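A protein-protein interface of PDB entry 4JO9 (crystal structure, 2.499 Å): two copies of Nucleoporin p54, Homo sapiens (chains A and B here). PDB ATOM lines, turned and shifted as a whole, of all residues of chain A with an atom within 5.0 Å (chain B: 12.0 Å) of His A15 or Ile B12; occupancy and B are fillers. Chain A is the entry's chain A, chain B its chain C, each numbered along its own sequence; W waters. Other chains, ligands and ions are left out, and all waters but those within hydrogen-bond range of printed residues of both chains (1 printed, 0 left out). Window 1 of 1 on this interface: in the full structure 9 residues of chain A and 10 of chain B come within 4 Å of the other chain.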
ATOM      1  N   LEU A   8     -21.443  25.946 -38.588  1.00  0.00           N
ATOM      2  CA  LEU A   8     -21.487  27.047 -37.635  1.00  0.00           C
ATOM      3  C   LEU A   8     -22.930  27.342 -37.239  1.00  0.00           C
ATOM      4  O   LEU A   8     -23.193  27.864 -36.156  1.00  0.00           O
ATOM      5  CB  LEU A   8     -20.829  28.294 -38.230  1.00  0.00           C
ATOM      6  CG  LEU A   8     -20.704  29.512 -37.313  1.00  0.00           C
ATOM      7  CD1 LEU A   8     -20.176  29.119 -35.942  1.00  0.00           C
ATOM      8  CD2 LEU A   8     -19.793  30.548 -37.951  1.00  0.00           C
ATOM      9  N   GLU A  11     -23.913  24.749 -34.685  1.00  0.00           N
ATOM     10  CA  GLU A  11     -23.241  25.111 -33.445  1.00  0.00           C
ATOM     11  C   GLU A  11     -24.031  26.186 -32.708  1.00  0.00           C
ATOM     12  O   GLU A  11     -24.263  26.085 -31.504  1.00  0.00           O
ATOM     13  CB  GLU A  11     -21.822  25.604 -33.735  1.00  0.00           C
ATOM     14  CG  GLU A  11     -20.863  24.503 -34.155  1.00  0.00           C
ATOM     15  CD  GLU A  11     -19.593  25.041 -34.785  1.00  0.00           C
ATOM     16  OE1 GLU A  11     -18.806  24.234 -35.324  1.00  0.00           O
ATOM     17  OE2 GLU A  11     -19.379  26.271 -34.739  1.00  0.00           O
ATOM     18  N   ILE A  12     -24.446  27.215 -33.442  1.00  0.00           N
ATOM     19  CA  ILE A  12     -25.237  28.296 -32.870  1.00  0.00           C
ATOM     20  C   ILE A  12     -26.570  27.771 -32.345  1.00  0.00           C
ATOM     21  O   ILE A  12     -26.958  28.070 -31.217  1.00  0.00           O
ATOM     22  CB  ILE A  12     -25.498  29.404 -33.907  1.00  0.00           C
ATOM     23  CG1 ILE A  12     -24.198  30.148 -34.218  1.00  0.00           C
ATOM     24  CG2 ILE A  12     -26.546  30.382 -33.390  1.00  0.00           C
ATOM     25  CD1 ILE A  12     -24.300  31.109 -35.385  1.00  0.00           C
ATOM     26  N   LYS A  13     -27.265  26.989 -33.165  1.00  0.00           N
ATOM     27  CA  LYS A  13     -28.547  26.415 -32.767  1.00  0.00           C
ATOM     28  C   LYS A  13     -28.410  25.606 -31.482  1.00  0.00           C
ATOM     29  O   LYS A  13     -29.256  25.692 -30.593  1.00  0.00           O
ATOM     30  CB  LYS A  13     -29.114  25.533 -33.881  1.00  0.00           C
ATOM     31  CG  LYS A  13     -30.222  26.195 -34.681  1.00  0.00           C
ATOM     32  CD  LYS A  13     -30.664  25.328 -35.847  1.00  0.00           C
ATOM     33  CE  LYS A  13     -31.456  26.134 -36.861  1.00  0.00           C
ATOM     34  NZ  LYS A  13     -31.930  25.298 -37.999  1.00  0.00           N
ATOM     35  N   GLN A  14     -27.340  24.825 -31.386  1.00  0.00           N
ATOM     36  CA  GLN A  14     -27.099  24.006 -30.206  1.00  0.00           C
ATOM     37  C   GLN A  14     -26.863  24.881 -28.980  1.00  0.00           C
ATOM     38  O   GLN A  14     -27.294  24.545 -27.878  1.00  0.00           O
ATOM     39  CB  GLN A  14     -25.892  23.093 -30.431  1.00  0.00           C
ATOM     40  CG  GLN A  14     -25.520  22.241 -29.227  1.00  0.00           C
ATOM     41  CD  GLN A  14     -26.669  21.390 -28.706  1.00  0.00           C
ATOM     42  OE1 GLN A  14     -26.694  21.029 -27.529  1.00  0.00           O
ATOM     43  NE2 GLN A  14     -27.618  21.058 -29.577  1.00  0.00           N
ATOM     44  N   HIS A  15     -26.171  25.998 -29.178  1.00  0.00           N
ATOM     45  CA  HIS A  15     -25.848  26.902 -28.084  1.00  0.00           C
ATOM     46  C   HIS A  15     -27.103  27.584 -27.550  1.00  0.00           C
ATOM     47  O   HIS A  15     -27.351  27.589 -26.345  1.00  0.00           O
ATOM     48  CB  HIS A  15     -24.843  27.960 -28.540  1.00  0.00           C
ATOM     49  CG  HIS A  15     -24.405  28.884 -27.446  1.00  0.00           C
ATOM     50  ND1 HIS A  15     -23.696  28.451 -26.345  1.00  0.00           N
ATOM     51  CD2 HIS A  15     -24.579  30.217 -27.281  1.00  0.00           C
ATOM     52  CE1 HIS A  15     -23.450  29.478 -25.552  1.00  0.00           C
ATOM     53  NE2 HIS A  15     -23.976  30.561 -26.096  1.00  0.00           N
ATOM     54  N   LEU A  16     -27.888  28.162 -28.453  1.00  0.00           N
ATOM     55  CA  LEU A  16     -29.121  28.838 -28.072  1.00  0.00           C
ATOM     56  C   LEU A  16     -30.082  27.860 -27.409  1.00  0.00           C
ATOM     57  O   LEU A  16     -30.794  28.215 -26.468  1.00  0.00           O
ATOM     58  CB  LEU A  16     -29.783  29.477 -29.295  1.00  0.00           C
ATOM     59  CG  LEU A  16     -28.959  30.546 -30.016  1.00  0.00           C
ATOM     60  CD1 LEU A  16     -29.781  31.198 -31.117  1.00  0.00           C
ATOM     61  CD2 LEU A  16     -28.441  31.594 -29.039  1.00  0.00           C
ATOM     62  N   LYS A  17     -30.102  26.627 -27.905  1.00  0.00           N
ATOM     63  CA  LYS A  17     -30.945  25.589 -27.328  1.00  0.00           C
ATOM     64  C   LYS A  17     -30.522  25.307 -25.890  1.00  0.00           C
ATOM     65  O   LYS A  17     -31.360  25.073 -25.021  1.00  0.00           O
ATOM     66  CB  LYS A  17     -30.860  24.311 -28.160  1.00  0.00           C
ATOM     67  CG  LYS A  17     -31.621  23.136 -27.571  1.00  0.00           C
ATOM     68  CD  LYS A  17     -31.342  21.853 -28.338  1.00  0.00           C
ATOM     69  CE  LYS A  17     -31.032  20.697 -27.400  1.00  0.00           C
ATOM     70  NZ  LYS A  17     -29.764  20.904 -26.640  1.00  0.00           N
ATOM     71  N   GLN A  18     -29.215  25.331 -25.648  1.00  0.00           N
ATOM     72  CA  GLN A  18     -28.681  25.118 -24.308  1.00  0.00           C
ATOM     73  C   GLN A  18     -29.107  26.242 -23.374  1.00  0.00           C
ATOM     74  O   GLN A  18     -29.358  26.014 -22.191  1.00  0.00           O
ATOM     75  CB  GLN A  18     -27.153  25.014 -24.346  1.00  0.00           C
ATOM     76  CG  GLN A  18     -26.640  23.602 -24.585  1.00  0.00           C
ATOM     77  CD  GLN A  18     -25.145  23.553 -24.840  1.00  0.00           C
ATOM     78  OE1 GLN A  18     -24.388  24.383 -24.335  1.00  0.00           O
ATOM     79  NE2 GLN A  18     -24.714  22.578 -25.631  1.00  0.00           N
ATOM     80  N   GLN A  19     -29.187  27.457 -23.908  1.00  0.00           N
ATOM     81  CA  GLN A  19     -29.637  28.595 -23.120  1.00  0.00           C
ATOM     82  C   GLN A  19     -31.096  28.415 -22.715  1.00  0.00           C
ATOM     83  O   GLN A  19     -31.459  28.641 -21.560  1.00  0.00           O
ATOM     84  CB  GLN A  19     -29.466  29.898 -23.900  1.00  0.00           C
ATOM     85  CG  GLN A  19     -28.028  30.353 -24.030  1.00  0.00           C
ATOM     86  CD  GLN A  19     -27.902  31.660 -24.782  1.00  0.00           C
ATOM     87  OE1 GLN A  19     -28.895  32.322 -25.076  1.00  0.00           O
ATOM     88  NE2 GLN A  19     -26.673  32.038 -25.101  1.00  0.00           N
ATOM     89  N   TYR B   2     -26.869  27.129 -13.792  1.00  0.00           N
ATOM     90  CA  TYR B   2     -27.183  26.821 -15.182  1.00  0.00           C
ATOM     91  C   TYR B   2     -25.981  26.210 -15.899  1.00  0.00           C
ATOM     92  O   TYR B   2     -24.885  26.772 -15.890  1.00  0.00           O
ATOM     93  CB  TYR B   2     -27.640  28.087 -15.910  1.00  0.00           C
ATOM     94  CG  TYR B   2     -26.594  29.174 -15.937  1.00  0.00           C
ATOM     95  CD1 TYR B   2     -26.370  29.979 -14.827  1.00  0.00           C
ATOM     96  CD2 TYR B   2     -25.824  29.392 -17.071  1.00  0.00           C
ATOM     97  CE1 TYR B   2     -25.410  30.973 -14.849  1.00  0.00           C
ATOM     98  CE2 TYR B   2     -24.863  30.384 -17.103  1.00  0.00           C
ATOM     99  CZ  TYR B   2     -24.660  31.171 -15.988  1.00  0.00           C
ATOM    100  OH  TYR B   2     -23.703  32.160 -16.011  1.00  0.00           O
ATOM    101  N   TYR B   3     -26.194  25.052 -16.514  1.00  0.00           N
ATOM    102  CA  TYR B   3     -25.143  24.382 -17.270  1.00  0.00           C
ATOM    103  C   TYR B   3     -25.151  24.812 -18.734  1.00  0.00           C
ATOM    104  O   TYR B   3     -26.164  24.690 -19.422  1.00  0.00           O
ATOM    105  CB  TYR B   3     -25.299  22.862 -17.186  1.00  0.00           C
ATOM    106  CG  TYR B   3     -24.444  22.119 -18.188  1.00  0.00           C
ATOM    107  CD1 TYR B   3     -24.900  21.886 -19.478  1.00  0.00           C
ATOM    108  CD2 TYR B   3     -23.177  21.660 -17.849  1.00  0.00           C
ATOM    109  CE1 TYR B   3     -24.124  21.214 -20.401  1.00  0.00           C
ATOM    110  CE2 TYR B   3     -22.393  20.985 -18.766  1.00  0.00           C
ATOM    111  CZ  TYR B   3     -22.871  20.765 -20.040  1.00  0.00           C
ATOM    112  OH  TYR B   3     -22.096  20.096 -20.959  1.00  0.00           O
ATOM    113  N   ILE B   4     -24.014  25.317 -19.201  1.00  0.00           N
ATOM    114  CA  ILE B   4     -23.843  25.645 -20.610  1.00  0.00           C
ATOM    115  C   ILE B   4     -22.413  25.330 -21.043  1.00  0.00           C
ATOM    116  O   ILE B   4     -21.454  25.661 -20.345  1.00  0.00           O
ATOM    117  CB  ILE B   4     -24.175  27.127 -20.897  1.00  0.00           C
ATOM    118  CG1 ILE B   4     -25.099  27.232 -22.113  1.00  0.00           C
ATOM    119  CG2 ILE B   4     -22.899  27.946 -21.092  1.00  0.00           C
ATOM    120  CD1 ILE B   4     -25.274  28.639 -22.641  1.00  0.00           C
ATOM    121  N   ASP B   5     -22.278  24.682 -22.196  1.00  0.00           N
ATOM    122  CA  ASP B   5     -20.973  24.248 -22.683  1.00  0.00           C
ATOM    123  C   ASP B   5     -20.133  25.444 -23.126  1.00  0.00           C
ATOM    124  O   ASP B   5     -20.481  26.140 -24.079  1.00  0.00           O
ATOM    125  CB  ASP B   5     -21.142  23.262 -23.842  1.00  0.00           C
ATOM    126  CG  ASP B   5     -19.845  22.575 -24.221  1.00  0.00           C
ATOM    127  OD1 ASP B   5     -18.780  23.222 -24.138  1.00  0.00           O
ATOM    128  OD2 ASP B   5     -19.889  21.385 -24.599  1.00  0.00           O
ATOM    129  N   ALA B   6     -19.026  25.676 -22.426  1.00  0.00           N
ATOM    130  CA  ALA B   6     -18.152  26.804 -22.728  1.00  0.00           C
ATOM    131  C   ALA B   6     -17.270  26.508 -23.937  1.00  0.00           C
ATOM    132  O   ALA B   6     -16.984  27.398 -24.739  1.00  0.00           O
ATOM    133  CB  ALA B   6     -17.297  27.147 -21.519  1.00  0.00           C
ATOM    134  N   ASP B   7     -16.839  25.257 -24.062  1.00  0.00           N
ATOM    135  CA  ASP B   7     -16.016  24.841 -25.194  1.00  0.00           C
ATOM    136  C   ASP B   7     -16.732  25.109 -26.514  1.00  0.00           C
ATOM    137  O   ASP B   7     -16.107  25.482 -27.505  1.00  0.00           O
ATOM    138  CB  ASP B   7     -15.662  23.356 -25.080  1.00  0.00           C
ATOM    139  CG  ASP B   7     -14.642  23.084 -23.994  1.00  0.00           C
ATOM    140  OD1 ASP B   7     -14.533  23.908 -23.060  1.00  0.00           O
ATOM    141  OD2 ASP B   7     -13.949  22.047 -24.073  1.00  0.00           O
ATOM    142  N   LEU B   8     -18.048  24.924 -26.517  1.00  0.00           N
ATOM    143  CA  LEU B   8     -18.847  25.148 -27.714  1.00  0.00           C
ATOM    144  C   LEU B   8     -18.963  26.636 -28.019  1.00  0.00           C
ATOM    145  O   LEU B   8     -19.004  27.037 -29.181  1.00  0.00           O
ATOM    146  CB  LEU B   8     -20.241  24.542 -27.542  1.00  0.00           C
ATOM    147  CG  LEU B   8     -21.242  24.830 -28.664  1.00  0.00           C
ATOM    148  CD1 LEU B   8     -20.710  24.351 -30.006  1.00  0.00           C
ATOM    149  CD2 LEU B   8     -22.583  24.184 -28.360  1.00  0.00           C
ATOM    150  N   LEU B   9     -19.014  27.451 -26.971  1.00  0.00           N
ATOM    151  CA  LEU B   9     -19.173  28.891 -27.137  1.00  0.00           C
ATOM    152  C   LEU B   9     -17.930  29.525 -27.754  1.00  0.00           C
ATOM    153  O   LEU B   9     -18.031  30.309 -28.697  1.00  0.00           O
ATOM    154  CB  LEU B   9     -19.490  29.554 -25.795  1.00  0.00           C
ATOM    155  CG  LEU B   9     -19.633  31.077 -25.839  1.00  0.00           C
ATOM    156  CD1 LEU B   9     -20.584  31.505 -26.948  1.00  0.00           C
ATOM    157  CD2 LEU B   9     -20.112  31.602 -24.494  1.00  0.00           C
ATOM    158  N   ARG B  10     -16.759  29.188 -27.224  1.00  0.00           N
ATOM    159  CA  ARG B  10     -15.511  29.707 -27.774  1.00  0.00           C
ATOM    160  C   ARG B  10     -15.251  29.109 -29.152  1.00  0.00           C
ATOM    161  O   ARG B  10     -14.565  29.710 -29.978  1.00  0.00           O
ATOM    162  CB  ARG B  10     -14.333  29.418 -26.840  1.00  0.00           C
ATOM    163  CG  ARG B  10     -14.097  27.946 -26.565  1.00  0.00           C
ATOM    164  CD  ARG B  10     -12.616  27.645 -26.417  1.00  0.00           C
ATOM    165  NE  ARG B  10     -12.372  26.227 -26.167  1.00  0.00           N
ATOM    166  CZ  ARG B  10     -12.436  25.277 -27.096  1.00  0.00           C
ATOM    167  NH1 ARG B  10     -12.744  25.580 -28.351  1.00  0.00           N
ATOM    168  NH2 ARG B  10     -12.196  24.015 -26.769  1.00  0.00           N
ATOM    169  N   GLU B  11     -15.800  27.924 -29.395  1.00  0.00           N
ATOM    170  CA  GLU B  11     -15.703  27.295 -30.706  1.00  0.00           C
ATOM    171  C   GLU B  11     -16.484  28.106 -31.735  1.00  0.00           C
ATOM    172  O   GLU B  11     -16.092  28.194 -32.897  1.00  0.00           O
ATOM    173  CB  GLU B  11     -16.233  25.861 -30.656  1.00  0.00           C
ATOM    174  CG  GLU B  11     -16.366  25.207 -32.021  1.00  0.00           C
ATOM    175  CD  GLU B  11     -16.901  23.792 -31.940  1.00  0.00           C
ATOM    176  OE1 GLU B  11     -17.159  23.193 -33.006  1.00  0.00           O
ATOM    177  OE2 GLU B  11     -17.065  23.279 -30.813  1.00  0.00           O
ATOM    178  N   ILE B  12     -17.593  28.693 -31.298  1.00  0.00           N
ATOM    179  CA  ILE B  12     -18.392  29.553 -32.162  1.00  0.00           C
ATOM    180  C   ILE B  12     -17.634  30.844 -32.459  1.00  0.00           C
ATOM    181  O   ILE B  12     -17.757  31.407 -33.546  1.00  0.00           O
ATOM    182  CB  ILE B  12     -19.759  29.885 -31.528  1.00  0.00           C
ATOM    183  CG1 ILE B  12     -20.654  28.643 -31.526  1.00  0.00           C
ATOM    184  CG2 ILE B  12     -20.445  31.016 -32.285  1.00  0.00           C
ATOM    185  CD1 ILE B  12     -21.986  28.839 -30.831  1.00  0.00           C
ATOM    186  N   LYS B  13     -16.846  31.306 -31.493  1.00  0.00           N
ATOM    187  CA  LYS B  13     -16.038  32.506 -31.681  1.00  0.00           C
ATOM    188  C   LYS B  13     -14.979  32.283 -32.757  1.00  0.00           C
ATOM    189  O   LYS B  13     -14.856  33.076 -33.691  1.00  0.00           O
ATOM    190  CB  LYS B  13     -15.368  32.921 -30.370  1.00  0.00           C
ATOM    191  CG  LYS B  13     -16.329  33.440 -29.315  1.00  0.00           C
ATOM    192  CD  LYS B  13     -15.579  34.007 -28.119  1.00  0.00           C
ATOM    193  CE  LYS B  13     -16.518  34.685 -27.134  1.00  0.00           C
ATOM    194  NZ  LYS B  13     -17.474  33.729 -26.510  1.00  0.00           N
ATOM    195  N   GLN B  14     -14.214  31.204 -32.619  1.00  0.00           N
ATOM    196  CA  GLN B  14     -13.175  30.871 -33.587  1.00  0.00           C
ATOM    197  C   GLN B  14     -13.728  30.893 -35.007  1.00  0.00           C
ATOM    198  O   GLN B  14     -13.205  31.589 -35.875  1.00  0.00           O
ATOM    199  CB  GLN B  14     -12.587  29.490 -33.291  1.00  0.00           C
ATOM    200  CG  GLN B  14     -11.735  29.425 -32.035  1.00  0.00           C
ATOM    201  CD  GLN B  14     -11.172  28.037 -31.792  1.00  0.00           C
ATOM    202  OE1 GLN B  14     -11.011  27.248 -32.723  1.00  0.00           O
ATOM    203  NE2 GLN B  14     -10.875  27.730 -30.534  1.00  0.00           N
ATOM    204  N   HIS B  15     -14.793  30.131 -35.232  1.00  0.00           N
ATOM    205  CA  HIS B  15     -15.381  30.000 -36.560  1.00  0.00           C
ATOM    206  C   HIS B  15     -15.810  31.350 -37.130  1.00  0.00           C
ATOM    207  O   HIS B  15     -15.846  31.533 -38.347  1.00  0.00           O
ATOM    208  CB  HIS B  15     -16.581  29.052 -36.521  1.00  0.00           C
ATOM    209  CG  HIS B  15     -16.215  27.621 -36.263  1.00  0.00           C
ATOM    210  ND1 HIS B  15     -14.983  27.240 -35.778  1.00  0.00           N
ATOM    211  CD2 HIS B  15     -16.924  26.479 -36.428  1.00  0.00           C
ATOM    212  CE1 HIS B  15     -14.949  25.925 -35.652  1.00  0.00           C
ATOM    213  NE2 HIS B  15     -16.113  25.439 -36.040  1.00  0.00           N
ATOM    214  N   LEU B  16     -16.134  32.292 -36.251  1.00  0.00           N
ATOM    215  CA  LEU B  16     -16.578  33.614 -36.679  1.00  0.00           C
ATOM    216  C   LEU B  16     -15.401  34.492 -37.097  1.00  0.00           C
ATOM    217  O   LEU B  16     -15.497  35.252 -38.060  1.00  0.00           O
ATOM    218  CB  LEU B  16     -17.376  34.294 -35.565  1.00  0.00           C
ATOM    219  CG  LEU B  16     -18.758  33.694 -35.297  1.00  0.00           C
ATOM    220  CD1 LEU B  16     -19.323  34.217 -33.986  1.00  0.00           C
ATOM    221  CD2 LEU B  16     -19.708  33.995 -36.444  1.00  0.00           C
ATOM    222  N   LYS B  17     -14.293  34.384 -36.372  1.00  0.00           N
ATOM    223  CA  LYS B  17     -13.096  35.156 -36.694  1.00  0.00           C
ATOM    224  C   LYS B  17     -12.402  34.596 -37.932  1.00  0.00           C
ATOM    225  O   LYS B  17     -11.992  35.347 -38.817  1.00  0.00           O
ATOM    226  CB  LYS B  17     -12.125  35.166 -35.512  1.00  0.00           C
ATOM    227  CG  LYS B  17     -12.674  35.848 -34.272  1.00  0.00           C
ATOM    228  CD  LYS B  17     -11.558  36.305 -33.347  1.00  0.00           C
ATOM    229  CE  LYS B  17     -12.082  37.245 -32.273  1.00  0.00           C
ATOM    230  NZ  LYS B  17     -10.985  37.821 -31.449  1.00  0.00           N
ATOM    231  N   GLN B  18     -12.273  33.275 -37.987  1.00  0.00           N
ATOM    232  CA  GLN B  18     -11.648  32.609 -39.125  1.00  0.00           C
ATOM    233  C   GLN B  18     -12.322  33.019 -40.427  1.00  0.00           C
ATOM    234  O   GLN B  18     -11.654  33.390 -41.393  1.00  0.00           O
ATOM    235  CB  GLN B  18     -11.725  31.090 -38.962  1.00  0.00           C
ATOM    236  CG  GLN B  18     -10.871  30.537 -37.832  1.00  0.00           C
ATOM    237  CD  GLN B  18     -11.176  29.082 -37.536  1.00  0.00           C
ATOM    238  OE1 GLN B  18     -11.997  28.459 -38.209  1.00  0.00           O
ATOM    239  NE2 GLN B  18     -10.517  28.533 -36.521  1.00  0.00           N
ATOM    240  N   GLN B  19     -13.647  32.952 -40.450  1.00  0.00           N
ATOM    241  CA  GLN B  19     -14.401  33.318 -41.641  1.00  0.00           C
ATOM    242  C   GLN B  19     -14.256  34.806 -41.932  1.00  0.00           C
ATOM    243  O   GLN B  19     -14.514  35.648 -41.071  1.00  0.00           O
ATOM    244  CB  GLN B  19     -15.872  32.965 -41.459  1.00  0.00           C
ATOM    245  CG  GLN B  19     -16.668  32.947 -42.744  1.00  0.00           C
ATOM    246  CD  GLN B  19     -18.128  32.663 -42.484  1.00  0.00           C
ATOM    247  OE1 GLN B  19     -18.521  32.378 -41.351  1.00  0.00           O
ATOM    248  NE2 GLN B  19     -18.945  32.746 -43.526  1.00  0.00           N
ATOM    249  N   GLN B  20     -13.849  35.115 -43.158  1.00  0.00           N
ATOM    250  CA  GLN B  20     -13.615  36.493 -43.578  1.00  0.00           C
ATOM    251  C   GLN B  20     -14.715  36.972 -44.519  1.00  0.00           C
ATOM    252  O   GLN B  20     -15.403  36.170 -45.151  1.00  0.00           O
ATOM    253  CB  GLN B  20     -12.247  36.630 -44.255  1.00  0.00           C
ATOM    254  CG  GLN B  20     -11.922  35.539 -45.277  1.00  0.00           C
ATOM    255  CD  GLN B  20     -10.604  35.775 -45.999  1.00  0.00           C
ATOM    256  OE1 GLN B  20     -10.541  35.730 -47.228  1.00  0.00           O
ATOM    257  NE2 GLN B  20      -9.543  36.015 -45.237  1.00  0.00           N
HETATM  258  O   HOH W   1     -28.721  23.574 -20.233  1.00  0.00           O
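A ring nitrogen (NE2) of His B15 is in hydrogen-bond range of the side-chain carboxylate (OE1) of Glu A11 (3.0 Å). The side-chain carboxylate of Glu A11 sits close to the side-chain carboxylate of Glu B11 (3.0 Å). N of Asp B5 lies within hydrogen-bond range of OE1 of Gln A18 (3.0 Å).
OE1 of Gln A14 is in hydrogen-bond range of NE2 of Gln A18, 3.1 Å away. A ring nitrogen (NE2) of His A15 is in hydrogen-bond range of the side-chain amide nitrogen of Gln A19, 3.2 Å away. O of Glu B11 is in hydrogen-bond range of ND1 of His B15 (3.2 Å). N of Asp B7 lies within hydrogen-bond range of OD1 of Asp B5, at 2.8 Å. OD1 of Asp B5 lies within hydrogen-bond range of N of Leu B8. OE1 of Gln A14 is in hydrogen-bond range of NZ of Lys A17, at 3.2 Å.
Among the printed residues, merely in contact across the chains: Gln A19 with Ile B4, His A15 with Ile B4, His A15 with Leu B9, Gln A14 with Leu B8, Glu A11 with Ile B12, Leu A8 with His B15, Gln A18 with Ile B4, Leu A8 with Leu B16, His A15 with Ile B12, Gln A18 with Leu B8 and Ile A12 with Ile B12.
Ile A12 touches just one residue of chain B: Ile B12. Of chain B, only Leu B8 comes within 4 Å of Gln A14. Lys A17 touches none of the printed residues of chain B. Gln A18 touches three residues of chain B. Of the printed residues of chain B, Gln A19 touches Ile B4 (3.5 Å). Of the printed residues of chain A, Leu B8 touches Gln A14 (3.6 Å) and Gln A18 (3.8 Å). Of the printed residues of chain A, Leu B9 touches His A15 (3.6 Å). Of chain A, only Glu A11 (3.6 Å), Ile A12 (3.9 Å) and His A15 (3.8 Å) come within 4 Å of Ile B12. Printed residues of chain A within 4 Å of His B15: Leu A8 and Glu A11. Of the printed residues of chain A, Leu B16 touches Leu A8. The nearest residue of chain A that does not touch Ile B12 is Leu A8 (4.1 Å). The nearest printed residue of chain A that does not touch Glu B11 is Leu A8 (5.2 Å).
Of the 10 printed residues of chain A, 7 touch a printed residue of chain B. Printed residues of chain A that touch a printed residue of chain B: Leu A8, Glu A11, Ile A12, Gln A14, His A15, Gln A18 and Gln A19. Along chain A the printed residues that touch a printed residue of chain B span positions 8 to 19. Among the printed residues, 14 pairs touch across the chains.
Leu A8 touches His B15, but with the chains exchanged His A15 does not touch Leu B8 (4.1 Å). Glu A11 touches Ile B12, but with the chains exchanged Ile A12 does not touch Glu B11 (8.2 Å). Glu A11 touches His B15, but with the chains exchanged His A15 does not touch Glu B11 (8.5 Å). His A15 touches Ile B12, but with the chains exchanged Ile A12 does not touch His B15 (8.0 Å). Positions printed for both chains: 8, 11, 12, 13, 14, 15, 16, 17, 18 and 19.
Water W1 lies within hydrogen-bond range of O of Tyr B3 (2.9 Å) and O of Gln A18 (3.2 Å).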
